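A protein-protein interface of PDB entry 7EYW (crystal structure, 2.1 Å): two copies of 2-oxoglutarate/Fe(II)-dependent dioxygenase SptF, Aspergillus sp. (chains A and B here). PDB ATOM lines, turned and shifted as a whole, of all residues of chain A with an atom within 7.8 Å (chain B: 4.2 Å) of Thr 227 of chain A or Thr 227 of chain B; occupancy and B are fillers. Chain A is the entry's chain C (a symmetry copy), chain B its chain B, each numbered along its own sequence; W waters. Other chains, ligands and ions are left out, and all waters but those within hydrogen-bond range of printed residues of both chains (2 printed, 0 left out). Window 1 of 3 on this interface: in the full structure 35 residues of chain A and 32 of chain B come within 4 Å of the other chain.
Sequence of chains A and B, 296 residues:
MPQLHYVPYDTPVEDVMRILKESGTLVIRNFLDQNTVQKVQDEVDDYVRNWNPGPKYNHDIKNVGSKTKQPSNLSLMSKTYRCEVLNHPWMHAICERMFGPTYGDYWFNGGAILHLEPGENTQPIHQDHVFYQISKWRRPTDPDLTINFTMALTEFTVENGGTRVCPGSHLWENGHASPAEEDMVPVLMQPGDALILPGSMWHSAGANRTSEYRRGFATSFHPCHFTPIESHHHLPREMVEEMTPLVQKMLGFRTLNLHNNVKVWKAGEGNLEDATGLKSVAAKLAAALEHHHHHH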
ATOM      1  N   TRP A 107      -4.776 -28.068 -12.362  1.00  0.00           N
ATOM      2  CA  TRP A 107      -4.576 -28.574 -11.011  1.00  0.00           C
ATOM      3  C   TRP A 107      -4.742 -27.448 -10.001  1.00  0.00           C
ATOM      4  O   TRP A 107      -4.873 -26.272 -10.352  1.00  0.00           O
ATOM      5  CB  TRP A 107      -3.216 -29.271 -10.843  1.00  0.00           C
ATOM      6  CG  TRP A 107      -1.985 -28.473 -11.197  1.00  0.00           C
ATOM      7  CD1 TRP A 107      -1.922 -27.304 -11.902  1.00  0.00           C
ATOM      8  CD2 TRP A 107      -0.632 -28.816 -10.871  1.00  0.00           C
ATOM      9  NE1 TRP A 107      -0.614 -26.897 -12.026  1.00  0.00           N
ATOM     10  CE2 TRP A 107       0.196 -27.808 -11.402  1.00  0.00           C
ATOM     11  CE3 TRP A 107      -0.043 -29.877 -10.176  1.00  0.00           C
ATOM     12  CZ2 TRP A 107       1.584 -27.833 -11.263  1.00  0.00           C
ATOM     13  CZ3 TRP A 107       1.334 -29.898 -10.037  1.00  0.00           C
ATOM     14  CH2 TRP A 107       2.131 -28.883 -10.576  1.00  0.00           C
ATOM     15  N   PHE A 108      -4.743 -27.843  -8.730  1.00  0.00           N
ATOM     16  CA  PHE A 108      -4.974 -26.920  -7.630  1.00  0.00           C
ATOM     17  C   PHE A 108      -3.922 -25.819  -7.622  1.00  0.00           C
ATOM     18  O   PHE A 108      -2.728 -26.077  -7.789  1.00  0.00           O
ATOM     19  CB  PHE A 108      -4.949 -27.696  -6.312  1.00  0.00           C
ATOM     20  CG  PHE A 108      -5.381 -26.904  -5.116  1.00  0.00           C
ATOM     21  CD1 PHE A 108      -6.713 -26.568  -4.935  1.00  0.00           C
ATOM     22  CD2 PHE A 108      -4.461 -26.524  -4.152  1.00  0.00           C
ATOM     23  CE1 PHE A 108      -7.115 -25.852  -3.826  1.00  0.00           C
ATOM     24  CE2 PHE A 108      -4.857 -25.807  -3.040  1.00  0.00           C
ATOM     25  CZ  PHE A 108      -6.186 -25.472  -2.877  1.00  0.00           C
ATOM     26  N   ASN A 109      -4.376 -24.579  -7.439  1.00  0.00           N
ATOM     27  CA  ASN A 109      -3.490 -23.421  -7.368  1.00  0.00           C
ATOM     28  C   ASN A 109      -3.251 -22.990  -5.925  1.00  0.00           C
ATOM     29  O   ASN A 109      -2.106 -22.934  -5.468  1.00  0.00           O
ATOM     30  CB  ASN A 109      -4.073 -22.262  -8.188  1.00  0.00           C
ATOM     31  CG  ASN A 109      -3.085 -21.126  -8.382  1.00  0.00           C
ATOM     32  OD1 ASN A 109      -1.897 -21.261  -8.090  1.00  0.00           O
ATOM     33  ND2 ASN A 109      -3.575 -19.998  -8.883  1.00  0.00           N
ATOM     34  N   GLY A 110      -4.321 -22.685  -5.198  1.00  0.00           N
ATOM     35  CA  GLY A 110      -4.201 -22.304  -3.806  1.00  0.00           C
ATOM     36  C   GLY A 110      -5.528 -22.239  -3.082  1.00  0.00           C
ATOM     37  O   GLY A 110      -6.560 -21.920  -3.681  1.00  0.00           O
ATOM     38  N   PHE A 131      -0.642 -11.625 -10.526  1.00  0.00           N
ATOM     39  CA  PHE A 131       0.671 -12.153 -10.179  1.00  0.00           C
ATOM     40  C   PHE A 131       1.199 -13.149 -11.206  1.00  0.00           C
ATOM     41  O   PHE A 131       2.259 -13.745 -10.986  1.00  0.00           O
ATOM     42  CB  PHE A 131       0.641 -12.783  -8.782  1.00  0.00           C
ATOM     43  CG  PHE A 131      -0.022 -14.127  -8.725  1.00  0.00           C
ATOM     44  CD1 PHE A 131      -1.394 -14.249  -8.880  1.00  0.00           C
ATOM     45  CD2 PHE A 131       0.726 -15.271  -8.498  1.00  0.00           C
ATOM     46  CE1 PHE A 131      -2.006 -15.484  -8.819  1.00  0.00           C
ATOM     47  CE2 PHE A 131       0.120 -16.512  -8.437  1.00  0.00           C
ATOM     48  CZ  PHE A 131      -1.247 -16.618  -8.599  1.00  0.00           C
ATOM     49  N   TYR A 132       0.488 -13.343 -12.315  1.00  0.00           N
ATOM     50  CA  TYR A 132       1.045 -14.004 -13.492  1.00  0.00           C
ATOM     51  C   TYR A 132       1.615 -12.919 -14.398  1.00  0.00           C
ATOM     52  O   TYR A 132       0.864 -12.104 -14.945  1.00  0.00           O
ATOM     53  CB  TYR A 132      -0.012 -14.824 -14.230  1.00  0.00           C
ATOM     54  CG  TYR A 132      -0.624 -15.967 -13.447  1.00  0.00           C
ATOM     55  CD1 TYR A 132      -1.722 -15.762 -12.621  1.00  0.00           C
ATOM     56  CD2 TYR A 132      -0.115 -17.256 -13.548  1.00  0.00           C
ATOM     57  CE1 TYR A 132      -2.290 -16.806 -11.913  1.00  0.00           C
ATOM     58  CE2 TYR A 132      -0.675 -18.306 -12.840  1.00  0.00           C
ATOM     59  CZ  TYR A 132      -1.762 -18.075 -12.024  1.00  0.00           C
ATOM     60  OH  TYR A 132      -2.323 -19.116 -11.318  1.00  0.00           O
ATOM     61  N   HIS A 222      -5.707 -23.735 -11.759  1.00  0.00           N
ATOM     62  CA  HIS A 222      -5.089 -23.071 -12.894  1.00  0.00           C
ATOM     63  C   HIS A 222      -4.436 -24.117 -13.772  1.00  0.00           C
ATOM     64  O   HIS A 222      -4.272 -25.278 -13.353  1.00  0.00           O
ATOM     65  CB  HIS A 222      -4.087 -21.995 -12.434  1.00  0.00           C
ATOM     66  CG  HIS A 222      -2.832 -22.534 -11.818  1.00  0.00           C
ATOM     67  ND1 HIS A 222      -1.744 -21.732 -11.549  1.00  0.00           N
ATOM     68  CD2 HIS A 222      -2.492 -23.778 -11.402  1.00  0.00           C
ATOM     69  CE1 HIS A 222      -0.785 -22.459 -11.005  1.00  0.00           C
ATOM     70  NE2 HIS A 222      -1.212 -23.705 -10.908  1.00  0.00           N
ATOM     71  N   PRO A 223      -4.083 -23.773 -15.015  1.00  0.00           N
ATOM     72  CA  PRO A 223      -3.515 -24.763 -15.935  1.00  0.00           C
ATOM     73  C   PRO A 223      -2.322 -25.504 -15.347  1.00  0.00           C
ATOM     74  O   PRO A 223      -1.571 -24.975 -14.525  1.00  0.00           O
ATOM     75  CB  PRO A 223      -3.098 -23.922 -17.143  1.00  0.00           C
ATOM     76  CG  PRO A 223      -4.067 -22.806 -17.150  1.00  0.00           C
ATOM     77  CD  PRO A 223      -4.392 -22.505 -15.712  1.00  0.00           C
ATOM     78  N   CYS A 224      -2.154 -26.748 -15.800  1.00  0.00           N
ATOM     79  CA  CYS A 224      -1.117 -27.619 -15.258  1.00  0.00           C
ATOM     80  C   CYS A 224       0.289 -27.119 -15.563  1.00  0.00           C
ATOM     81  O   CYS A 224       1.232 -27.505 -14.865  1.00  0.00           O
ATOM     82  CB  CYS A 224      -1.293 -29.039 -15.799  1.00  0.00           C
ATOM     83  SG  CYS A 224      -1.075 -29.192 -17.589  1.00  0.00           S
ATOM     84  N   HIS A 225       0.456 -26.279 -16.582  1.00  0.00           N
ATOM     85  CA  HIS A 225       1.773 -25.750 -16.915  1.00  0.00           C
ATOM     86  C   HIS A 225       2.157 -24.537 -16.078  1.00  0.00           C
ATOM     87  O   HIS A 225       3.218 -23.951 -16.320  1.00  0.00           O
ATOM     88  CB  HIS A 225       1.842 -25.390 -18.401  1.00  0.00           C
ATOM     89  CG  HIS A 225       3.165 -25.694 -19.032  1.00  0.00           C
ATOM     90  ND1 HIS A 225       3.360 -25.680 -20.397  1.00  0.00           N
ATOM     91  CD2 HIS A 225       4.359 -26.022 -18.484  1.00  0.00           C
ATOM     92  CE1 HIS A 225       4.617 -25.987 -20.662  1.00  0.00           C
ATOM     93  NE2 HIS A 225       5.246 -26.197 -19.519  1.00  0.00           N
ATOM     94  N   PHE A 226       1.332 -24.147 -15.111  1.00  0.00           N
ATOM     95  CA  PHE A 226       1.629 -23.039 -14.217  1.00  0.00           C
ATOM     96  C   PHE A 226       1.920 -23.575 -12.822  1.00  0.00           C
ATOM     97  O   PHE A 226       1.303 -24.551 -12.380  1.00  0.00           O
ATOM     98  CB  PHE A 226       0.467 -22.039 -14.162  1.00  0.00           C
ATOM     99  CG  PHE A 226       0.107 -21.441 -15.497  1.00  0.00           C
ATOM    100  CD1 PHE A 226       1.021 -21.417 -16.539  1.00  0.00           C
ATOM    101  CD2 PHE A 226      -1.150 -20.898 -15.705  1.00  0.00           C
ATOM    102  CE1 PHE A 226       0.685 -20.867 -17.764  1.00  0.00           C
ATOM    103  CE2 PHE A 226      -1.491 -20.345 -16.927  1.00  0.00           C
ATOM    104  CZ  PHE A 226      -0.573 -20.331 -17.957  1.00  0.00           C
ATOM    105  N   THR A 227       2.858 -22.938 -12.132  1.00  0.00           N
ATOM    106  CA  THR A 227       3.264 -23.401 -10.811  1.00  0.00           C
ATOM    107  C   THR A 227       2.250 -22.956  -9.766  1.00  0.00           C
ATOM    108  O   THR A 227       1.987 -21.754  -9.646  1.00  0.00           O
ATOM    109  CB  THR A 227       4.644 -22.873 -10.456  1.00  0.00           C
ATOM    110  OG1 THR A 227       5.550 -23.148 -11.532  1.00  0.00           O
ATOM    111  CG2 THR A 227       5.160 -23.535  -9.185  1.00  0.00           C
ATOM    112  N   PRO A 228       1.673 -23.871  -8.992  1.00  0.00           N
ATOM    113  CA  PRO A 228       0.660 -23.475  -8.010  1.00  0.00           C
ATOM    114  C   PRO A 228       1.257 -22.655  -6.878  1.00  0.00           C
ATOM    115  O   PRO A 228       2.446 -22.750  -6.564  1.00  0.00           O
ATOM    116  CB  PRO A 228       0.115 -24.810  -7.494  1.00  0.00           C
ATOM    117  CG  PRO A 228       1.164 -25.808  -7.801  1.00  0.00           C
ATOM    118  CD  PRO A 228       1.910 -25.324  -9.003  1.00  0.00           C
ATOM    119  N   ILE A 229       0.400 -21.835  -6.268  1.00  0.00           N
ATOM    120  CA  ILE A 229       0.809 -21.038  -5.116  1.00  0.00           C
ATOM    121  C   ILE A 229       1.286 -21.943  -3.988  1.00  0.00           C
ATOM    122  O   ILE A 229       2.272 -21.644  -3.303  1.00  0.00           O
ATOM    123  CB  ILE A 229      -0.354 -20.134  -4.663  1.00  0.00           C
ATOM    124  CG1 ILE A 229      -0.590 -19.016  -5.679  1.00  0.00           C
ATOM    125  CG2 ILE A 229      -0.092 -19.559  -3.282  1.00  0.00           C
ATOM    126  CD1 ILE A 229      -2.047 -18.642  -5.831  1.00  0.00           C
ATOM    127  N   GLU A 230       0.610 -23.070  -3.793  1.00  0.00           N
ATOM    128  CA  GLU A 230       0.866 -23.959  -2.672  1.00  0.00           C
ATOM    129  C   GLU A 230       1.448 -25.276  -3.166  1.00  0.00           C
ATOM    130  O   GLU A 230       0.963 -25.845  -4.149  1.00  0.00           O
ATOM    131  CB  GLU A 230      -0.420 -24.227  -1.888  1.00  0.00           C
ATOM    132  CG  GLU A 230      -1.112 -22.980  -1.375  1.00  0.00           C
ATOM    133  CD  GLU A 230      -2.290 -23.310  -0.486  1.00  0.00           C
ATOM    134  OE1 GLU A 230      -2.684 -24.495  -0.446  1.00  0.00           O
ATOM    135  OE2 GLU A 230      -2.822 -22.391   0.172  1.00  0.00           O
ATOM    136  N   SER A 231       2.485 -25.748  -2.487  1.00  0.00           N
ATOM    137  CA  SER A 231       2.966 -27.111  -2.636  1.00  0.00           C
ATOM    138  C   SER A 231       2.368 -27.973  -1.534  1.00  0.00           C
ATOM    139  O   SER A 231       2.097 -27.497  -0.428  1.00  0.00           O
ATOM    140  CB  SER A 231       4.494 -27.166  -2.579  1.00  0.00           C
ATOM    141  OG  SER A 231       4.951 -28.507  -2.529  1.00  0.00           O
ATOM    142  N   LEU A 256       1.114 -34.621 -15.170  1.00  0.00           N
ATOM    143  CA  LEU A 256       0.089 -33.851 -15.856  1.00  0.00           C
ATOM    144  C   LEU A 256       0.287 -33.906 -17.366  1.00  0.00           C
ATOM    145  O   LEU A 256       1.415 -33.970 -17.862  1.00  0.00           O
ATOM    146  CB  LEU A 256       0.103 -32.400 -15.380  1.00  0.00           C
ATOM    147  CG  LEU A 256       0.059 -32.239 -13.859  1.00  0.00           C
ATOM    148  CD1 LEU A 256       0.951 -31.092 -13.414  1.00  0.00           C
ATOM    149  CD2 LEU A 256      -1.369 -32.031 -13.382  1.00  0.00           C
ATOM    150  N   LEU A 258      -0.300 -32.073 -20.968  1.00  0.00           N
ATOM    151  CA  LEU A 258      -0.632 -30.889 -21.743  1.00  0.00           C
ATOM    152  C   LEU A 258      -1.618 -31.256 -22.853  1.00  0.00           C
ATOM    153  O   LEU A 258      -1.951 -32.426 -23.065  1.00  0.00           O
ATOM    154  CB  LEU A 258       0.632 -30.255 -22.324  1.00  0.00           C
ATOM    155  CG  LEU A 258       1.639 -29.705 -21.311  1.00  0.00           C
ATOM    156  CD1 LEU A 258       2.848 -29.121 -22.022  1.00  0.00           C
ATOM    157  CD2 LEU A 258       0.991 -28.659 -20.420  1.00  0.00           C
ATOM    158  N   LYS A 263       3.726 -34.478 -21.656  1.00  0.00           N
ATOM    159  CA  LYS A 263       3.647 -34.610 -20.211  1.00  0.00           C
ATOM    160  C   LYS A 263       4.605 -33.640 -19.534  1.00  0.00           C
ATOM    161  O   LYS A 263       5.740 -33.451 -19.981  1.00  0.00           O
ATOM    162  CB  LYS A 263       3.964 -36.040 -19.771  1.00  0.00           C
ATOM    163  CG  LYS A 263       3.177 -37.113 -20.500  1.00  0.00           C
ATOM    164  CD  LYS A 263       3.706 -38.498 -20.165  1.00  0.00           C
ATOM    165  CE  LYS A 263       5.089 -38.722 -20.758  1.00  0.00           C
ATOM    166  NZ  LYS A 263       5.150 -38.317 -22.190  1.00  0.00           N
ATOM    167  N   VAL A 264       4.129 -33.016 -18.459  1.00  0.00           N
ATOM    168  CA  VAL A 264       4.965 -32.257 -17.542  1.00  0.00           C
ATOM    169  C   VAL A 264       4.819 -32.884 -16.161  1.00  0.00           C
ATOM    170  O   VAL A 264       3.973 -33.750 -15.939  1.00  0.00           O
ATOM    171  CB  VAL A 264       4.603 -30.760 -17.511  1.00  0.00           C
ATOM    172  CG1 VAL A 264       4.901 -30.114 -18.857  1.00  0.00           C
ATOM    173  CG2 VAL A 264       3.142 -30.577 -17.136  1.00  0.00           C
ATOM    174  N   TRP A 265       5.663 -32.436 -15.230  1.00  0.00           N
ATOM    175  CA  TRP A 265       5.684 -32.985 -13.872  1.00  0.00           C
ATOM    176  C   TRP A 265       5.966 -34.487 -13.902  1.00  0.00           C
ATOM    177  O   TRP A 265       5.324 -35.274 -13.204  1.00  0.00           O
ATOM    178  CB  TRP A 265       4.374 -32.679 -13.137  1.00  0.00           C
ATOM    179  CG  TRP A 265       4.481 -32.547 -11.643  1.00  0.00           C
ATOM    180  CD1 TRP A 265       3.699 -33.167 -10.712  1.00  0.00           C
ATOM    181  CD2 TRP A 265       5.405 -31.730 -10.907  1.00  0.00           C
ATOM    182  NE1 TRP A 265       4.081 -32.797  -9.447  1.00  0.00           N
ATOM    183  CE2 TRP A 265       5.126 -31.916  -9.538  1.00  0.00           C
ATOM    184  CE3 TRP A 265       6.441 -30.863 -11.272  1.00  0.00           C
ATOM    185  CZ2 TRP A 265       5.845 -31.269  -8.534  1.00  0.00           C
ATOM    186  CZ3 TRP A 265       7.155 -30.224 -10.273  1.00  0.00           C
ATOM    187  CH2 TRP A 265       6.854 -30.429  -8.922  1.00  0.00           C
ATOM    188  N   LYS A 266       6.930 -34.882 -14.728  1.00  0.00           N
ATOM    189  CA  LYS A 266       7.255 -36.282 -14.954  1.00  0.00           C
ATOM    190  C   LYS A 266       8.293 -36.774 -13.954  1.00  0.00           C
ATOM    191  O   LYS A 266       8.985 -35.994 -13.294  1.00  0.00           O
ATOM    192  CB  LYS A 266       7.791 -36.493 -16.372  1.00  0.00           C
ATOM    193  CG  LYS A 266       6.764 -36.366 -17.480  1.00  0.00           C
ATOM    194  CD  LYS A 266       7.420 -35.877 -18.766  1.00  0.00           C
ATOM    195  CE  LYS A 266       8.809 -36.471 -18.944  1.00  0.00           C
ATOM    196  NZ  LYS A 266       9.503 -35.949 -20.153  1.00  0.00           N
ATOM    197  N   TRP B 107      13.775 -22.034 -12.129  1.00  0.00           N
ATOM    198  CA  TRP B 107      14.134 -23.345 -11.612  1.00  0.00           C
ATOM    199  C   TRP B 107      14.272 -24.334 -12.760  1.00  0.00           C
ATOM    200  O   TRP B 107      13.966 -24.034 -13.918  1.00  0.00           O
ATOM    201  CB  TRP B 107      13.126 -23.849 -10.565  1.00  0.00           C
ATOM    202  CG  TRP B 107      11.686 -23.942 -11.001  1.00  0.00           C
ATOM    203  CD1 TRP B 107      11.127 -23.440 -12.142  1.00  0.00           C
ATOM    204  CD2 TRP B 107      10.622 -24.579 -10.281  1.00  0.00           C
ATOM    205  NE1 TRP B 107       9.782 -23.727 -12.176  1.00  0.00           N
ATOM    206  CE2 TRP B 107       9.448 -24.427 -11.046  1.00  0.00           C
ATOM    207  CE3 TRP B 107      10.549 -25.267  -9.065  1.00  0.00           C
ATOM    208  CZ2 TRP B 107       8.216 -24.933 -10.631  1.00  0.00           C
ATOM    209  CZ3 TRP B 107       9.325 -25.770  -8.657  1.00  0.00           C
ATOM    210  CH2 TRP B 107       8.177 -25.601  -9.439  1.00  0.00           C
ATOM    211  N   HIS B 222      13.597 -22.541 -16.549  1.00  0.00           N
ATOM    212  CA  HIS B 222      12.504 -21.688 -16.995  1.00  0.00           C
ATOM    213  C   HIS B 222      11.921 -20.980 -15.779  1.00  0.00           C
ATOM    214  O   HIS B 222      12.220 -21.354 -14.635  1.00  0.00           O
ATOM    215  CB  HIS B 222      11.436 -22.499 -17.759  1.00  0.00           C
ATOM    216  CG  HIS B 222      10.644 -23.451 -16.914  1.00  0.00           C
ATOM    217  ND1 HIS B 222       9.554 -24.136 -17.407  1.00  0.00           N
ATOM    218  CD2 HIS B 222      10.785 -23.848 -15.627  1.00  0.00           C
ATOM    219  CE1 HIS B 222       9.053 -24.905 -16.458  1.00  0.00           C
ATOM    220  NE2 HIS B 222       9.779 -24.747 -15.367  1.00  0.00           N
ATOM    221  N   CYS B 224       9.989 -19.613 -12.552  1.00  0.00           N
ATOM    222  CA  CYS B 224       9.463 -20.398 -11.442  1.00  0.00           C
ATOM    223  C   CYS B 224       7.948 -20.524 -11.480  1.00  0.00           C
ATOM    224  O   CYS B 224       7.400 -21.426 -10.841  1.00  0.00           O
ATOM    225  CB  CYS B 224       9.896 -19.782 -10.112  1.00  0.00           C
ATOM    226  SG  CYS B 224       9.228 -18.134  -9.804  1.00  0.00           S
ATOM    227  N   HIS B 225       7.257 -19.641 -12.202  1.00  0.00           N
ATOM    228  CA  HIS B 225       5.810 -19.743 -12.341  1.00  0.00           C
ATOM    229  C   HIS B 225       5.386 -20.755 -13.396  1.00  0.00           C
ATOM    230  O   HIS B 225       4.182 -20.902 -13.638  1.00  0.00           O
ATOM    231  CB  HIS B 225       5.211 -18.373 -12.674  1.00  0.00           C
ATOM    232  CG  HIS B 225       3.911 -18.096 -11.983  1.00  0.00           C
ATOM    233  ND1 HIS B 225       3.428 -16.819 -11.795  1.00  0.00           N
ATOM    234  CD2 HIS B 225       2.995 -18.929 -11.436  1.00  0.00           C
ATOM    235  CE1 HIS B 225       2.270 -16.878 -11.161  1.00  0.00           C
ATOM    236  NE2 HIS B 225       1.984 -18.147 -10.931  1.00  0.00           N
ATOM    237  N   PHE B 226       6.330 -21.448 -14.028  1.00  0.00           N
ATOM    238  CA  PHE B 226       6.030 -22.466 -15.025  1.00  0.00           C
ATOM    239  C   PHE B 226       6.316 -23.847 -14.451  1.00  0.00           C
ATOM    240  O   PHE B 226       7.314 -24.045 -13.749  1.00  0.00           O
ATOM    241  CB  PHE B 226       6.850 -22.257 -16.306  1.00  0.00           C
ATOM    242  CG  PHE B 226       6.618 -20.927 -16.979  1.00  0.00           C
ATOM    243  CD1 PHE B 226       5.492 -20.166 -16.701  1.00  0.00           C
ATOM    244  CD2 PHE B 226       7.530 -20.444 -17.903  1.00  0.00           C
ATOM    245  CE1 PHE B 226       5.288 -18.948 -17.325  1.00  0.00           C
ATOM    246  CE2 PHE B 226       7.331 -19.230 -18.531  1.00  0.00           C
ATOM    247  CZ  PHE B 226       6.209 -18.481 -18.241  1.00  0.00           C
ATOM    248  N   THR B 227       5.440 -24.797 -14.752  1.00  0.00           N
ATOM    249  CA  THR B 227       5.608 -26.152 -14.239  1.00  0.00           C
ATOM    250  C   THR B 227       6.736 -26.856 -14.985  1.00  0.00           C
ATOM    251  O   THR B 227       6.744 -26.865 -16.222  1.00  0.00           O
ATOM    252  CB  THR B 227       4.310 -26.943 -14.380  1.00  0.00           C
ATOM    253  OG1 THR B 227       3.255 -26.255 -13.698  1.00  0.00           O
ATOM    254  CG2 THR B 227       4.463 -28.342 -13.796  1.00  0.00           C
ATOM    255  N   PRO B 228       7.695 -27.455 -14.283  1.00  0.00           N
ATOM    256  CA  PRO B 228       8.797 -28.128 -14.973  1.00  0.00           C
ATOM    257  C   PRO B 228       8.327 -29.397 -15.662  1.00  0.00           C
ATOM    258  O   PRO B 228       7.327 -30.011 -15.279  1.00  0.00           O
ATOM    259  CB  PRO B 228       9.789 -28.450 -13.845  1.00  0.00           C
ATOM    260  CG  PRO B 228       9.304 -27.687 -12.641  1.00  0.00           C
ATOM    261  CD  PRO B 228       7.833 -27.528 -12.820  1.00  0.00           C
ATOM    262  N   ILE B 229       9.067 -29.780 -16.704  1.00  0.00           N
ATOM    263  CA  ILE B 229       8.814 -31.053 -17.373  1.00  0.00           C
ATOM    264  C   ILE B 229       8.961 -32.203 -16.385  1.00  0.00           C
ATOM    265  O   ILE B 229       8.176 -33.159 -16.394  1.00  0.00           O
ATOM    266  CB  ILE B 229       9.759 -31.215 -18.581  1.00  0.00           C
ATOM    267  CG1 ILE B 229       9.249 -30.406 -19.779  1.00  0.00           C
ATOM    268  CG2 ILE B 229       9.941 -32.687 -18.939  1.00  0.00           C
ATOM    269  CD1 ILE B 229       8.304 -31.172 -20.688  1.00  0.00           C
ATOM    270  N   TRP B 265       4.714 -22.002  -4.752  1.00  0.00           N
ATOM    271  CA  TRP B 265       5.272 -23.260  -4.250  1.00  0.00           C
ATOM    272  C   TRP B 265       5.453 -23.204  -2.733  1.00  0.00           C
ATOM    273  O   TRP B 265       6.458 -23.663  -2.189  1.00  0.00           O
ATOM    274  CB  TRP B 265       6.591 -23.599  -4.954  1.00  0.00           C
ATOM    275  CG  TRP B 265       6.873 -25.067  -5.104  1.00  0.00           C
ATOM    276  CD1 TRP B 265       8.016 -25.720  -4.741  1.00  0.00           C
ATOM    277  CD2 TRP B 265       6.008 -26.062  -5.671  1.00  0.00           C
ATOM    278  NE1 TRP B 265       7.914 -27.057  -5.039  1.00  0.00           N
ATOM    279  CE2 TRP B 265       6.692 -27.293  -5.610  1.00  0.00           C
ATOM    280  CE3 TRP B 265       4.722 -26.033  -6.221  1.00  0.00           C
ATOM    281  CZ2 TRP B 265       6.134 -28.481  -6.078  1.00  0.00           C
ATOM    282  CZ3 TRP B 265       4.170 -27.214  -6.682  1.00  0.00           C
ATOM    283  CH2 TRP B 265       4.875 -28.420  -6.609  1.00  0.00           C
HETATM  284  O   HOH W   1       7.737 -27.055 -18.701  1.00  0.00           O
HETATM  285  O   HOH W   2       0.227 -19.714  -9.131  1.00  0.00           O
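The side-chain hydroxyl (OG1) of Thr 227 of chain A sits at hydrogen-bond distance from the backbone carbonyl oxygen (O) of Cys 224 of chain B (2.6 Å).
ND1 of His 225 of chain B sits close to O of Phe 131 of chain A, at 3.4 Å.
N of Thr 227 of chain A sits at hydrogen-bond distance from O of His 225 of chain B (2.9 Å).
The backbone carbonyl oxygen (O) of Phe 226 of chain B lies within hydrogen-bond range of the side-chain hydroxyl (OG1) of Thr 227 of chain A, 3.0 Å away.
O of Cys 224 of chain A is in hydrogen-bond range of OG1 of Thr 227 of chain B (2.6 Å).
N of Thr 227 of chain B sits at hydrogen-bond distance from O of His 225 of chain A (2.8 Å).
OG1 of Thr 227 of chain B lies within hydrogen-bond range of O of Phe 226 of chain A, at 2.9 Å.
The backbone carbonyl oxygen of Pro 228 of chain B sits at hydrogen-bond distance from the backbone NH of Trp 265 of chain A (2.9 Å).
The backbone carbonyl oxygen (O) of Ile 229 of chain B is in hydrogen-bond range of the backbone NH (N) of Trp 265 of chain A, 2.9 Å away.
The backbone NH (N) of Lys 266 of chain A is in hydrogen-bond range of the backbone carbonyl oxygen (O) of Ile 229 of chain B, at 2.7 Å.
The backbone NH (N) of Trp 265 of chain B is in hydrogen-bond range of the backbone carbonyl oxygen (O) of Pro 228 of chain A.
The backbone carbonyl oxygen of Ile 229 of chain A sits at hydrogen-bond distance from the backbone NH of Trp 265 of chain B (2.9 Å).
The indole nitrogen (NE1) of Trp 107 of chain A sits at hydrogen-bond distance from the backbone carbonyl oxygen (O) of Pro 223 of chain A (3.3 Å).
The backbone carbonyl oxygen (O) of Asn 109 of chain A lies within hydrogen-bond range of the backbone NH (N) of Ile 229 of chain A, at 2.9 Å.
A ring nitrogen (NE2) of His 222 of chain A is in hydrogen-bond range of the backbone carbonyl oxygen (O) of Phe 226 of chain A.
Trp 107 of chain A touches Thr 227 of chain B.
NE2 of His 225 of chain B touches CE2 of Tyr 132 of chain A, 3.3 Å away.
O of His 225 of chain B touches CA of Phe 226 of chain A, at 3.4 Å.
Thr 227 of chain A touches Trp 107 of chain B (OG1 to CZ2, 3.3 Å).
CG2 of Thr 227 of chain A touches CE3 of Trp 265 of chain B, at 3.9 Å.
Trp 265 of chain B touches Ser 231 of chain A.
Lys 263 of chain A touches Ile 229 of chain B (O to CD1, 3.5 Å).
Val 264 of chain A touches Pro 228 of chain B.
Ile 229 of chain B touches Val 264 of chain A.
Of the printed residues of chain B, Tyr 132 of chain A touches His 225.
Of the printed residues of chain B, Phe 226 of chain A touches His 225 (3.4 Å) and Thr 227 (2.9 Å).
Of the printed residues of chain B, Thr 227 of chain A touches Trp 107, Cys 224, His 225, Phe 226, Thr 227 and Trp 265.
Leu 256 of chain A touches none of the printed residues of chain B.
Of the printed residues of chain A, Trp 107 of chain B touches Thr 227.
Pro 228 of chain B touches two residues of chain A.
Printed residues of chain A within 4 Å of Ile 229 of chain B: Lys 263, Val 264, Trp 265 and Lys 266.
The nearest printed residue of chain B that does not touch Thr 227 of chain A is Pro 228 of chain B (5.1 Å).
The nearest printed residue of chain B that does not touch Val 264 of chain A is Thr 227 of chain B (4.2 Å).
Of the 22 printed residues of chain A, 14 touch a printed residue of chain B.
Trp 107 of chain A touches Thr 227 of chain B, and with the chains exchanged Thr 227 of chain A touches Trp 107 of chain B.
His 225 of chain A touches Thr 227 of chain B, and with the chains exchanged Thr 227 of chain A touches His 225 of chain B.
Thr 227 of chain A touches Trp 265 of chain B, but with the chains exchanged Trp 265 of chain A does not touch Thr 227 of chain B (4.1 Å).
Pro 228 of chain A touches Trp 265 of chain B, and with the chains exchanged Trp 265 of chain A touches Pro 228 of chain B.
Water W1 bridges O of Thr 227 of chain B (2.7 Å) and NE2 of His 225 of chain A (2.8 Å).
Water W2 lies within hydrogen-bond range of the backbone carbonyl oxygen of Thr 227 of chain A, the side-chain amide oxygen of Asn 109 of chain A, a ring nitrogen (NE2) of His 225 of chain B and the side-chain hydroxyl of Tyr 132 of chain A.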
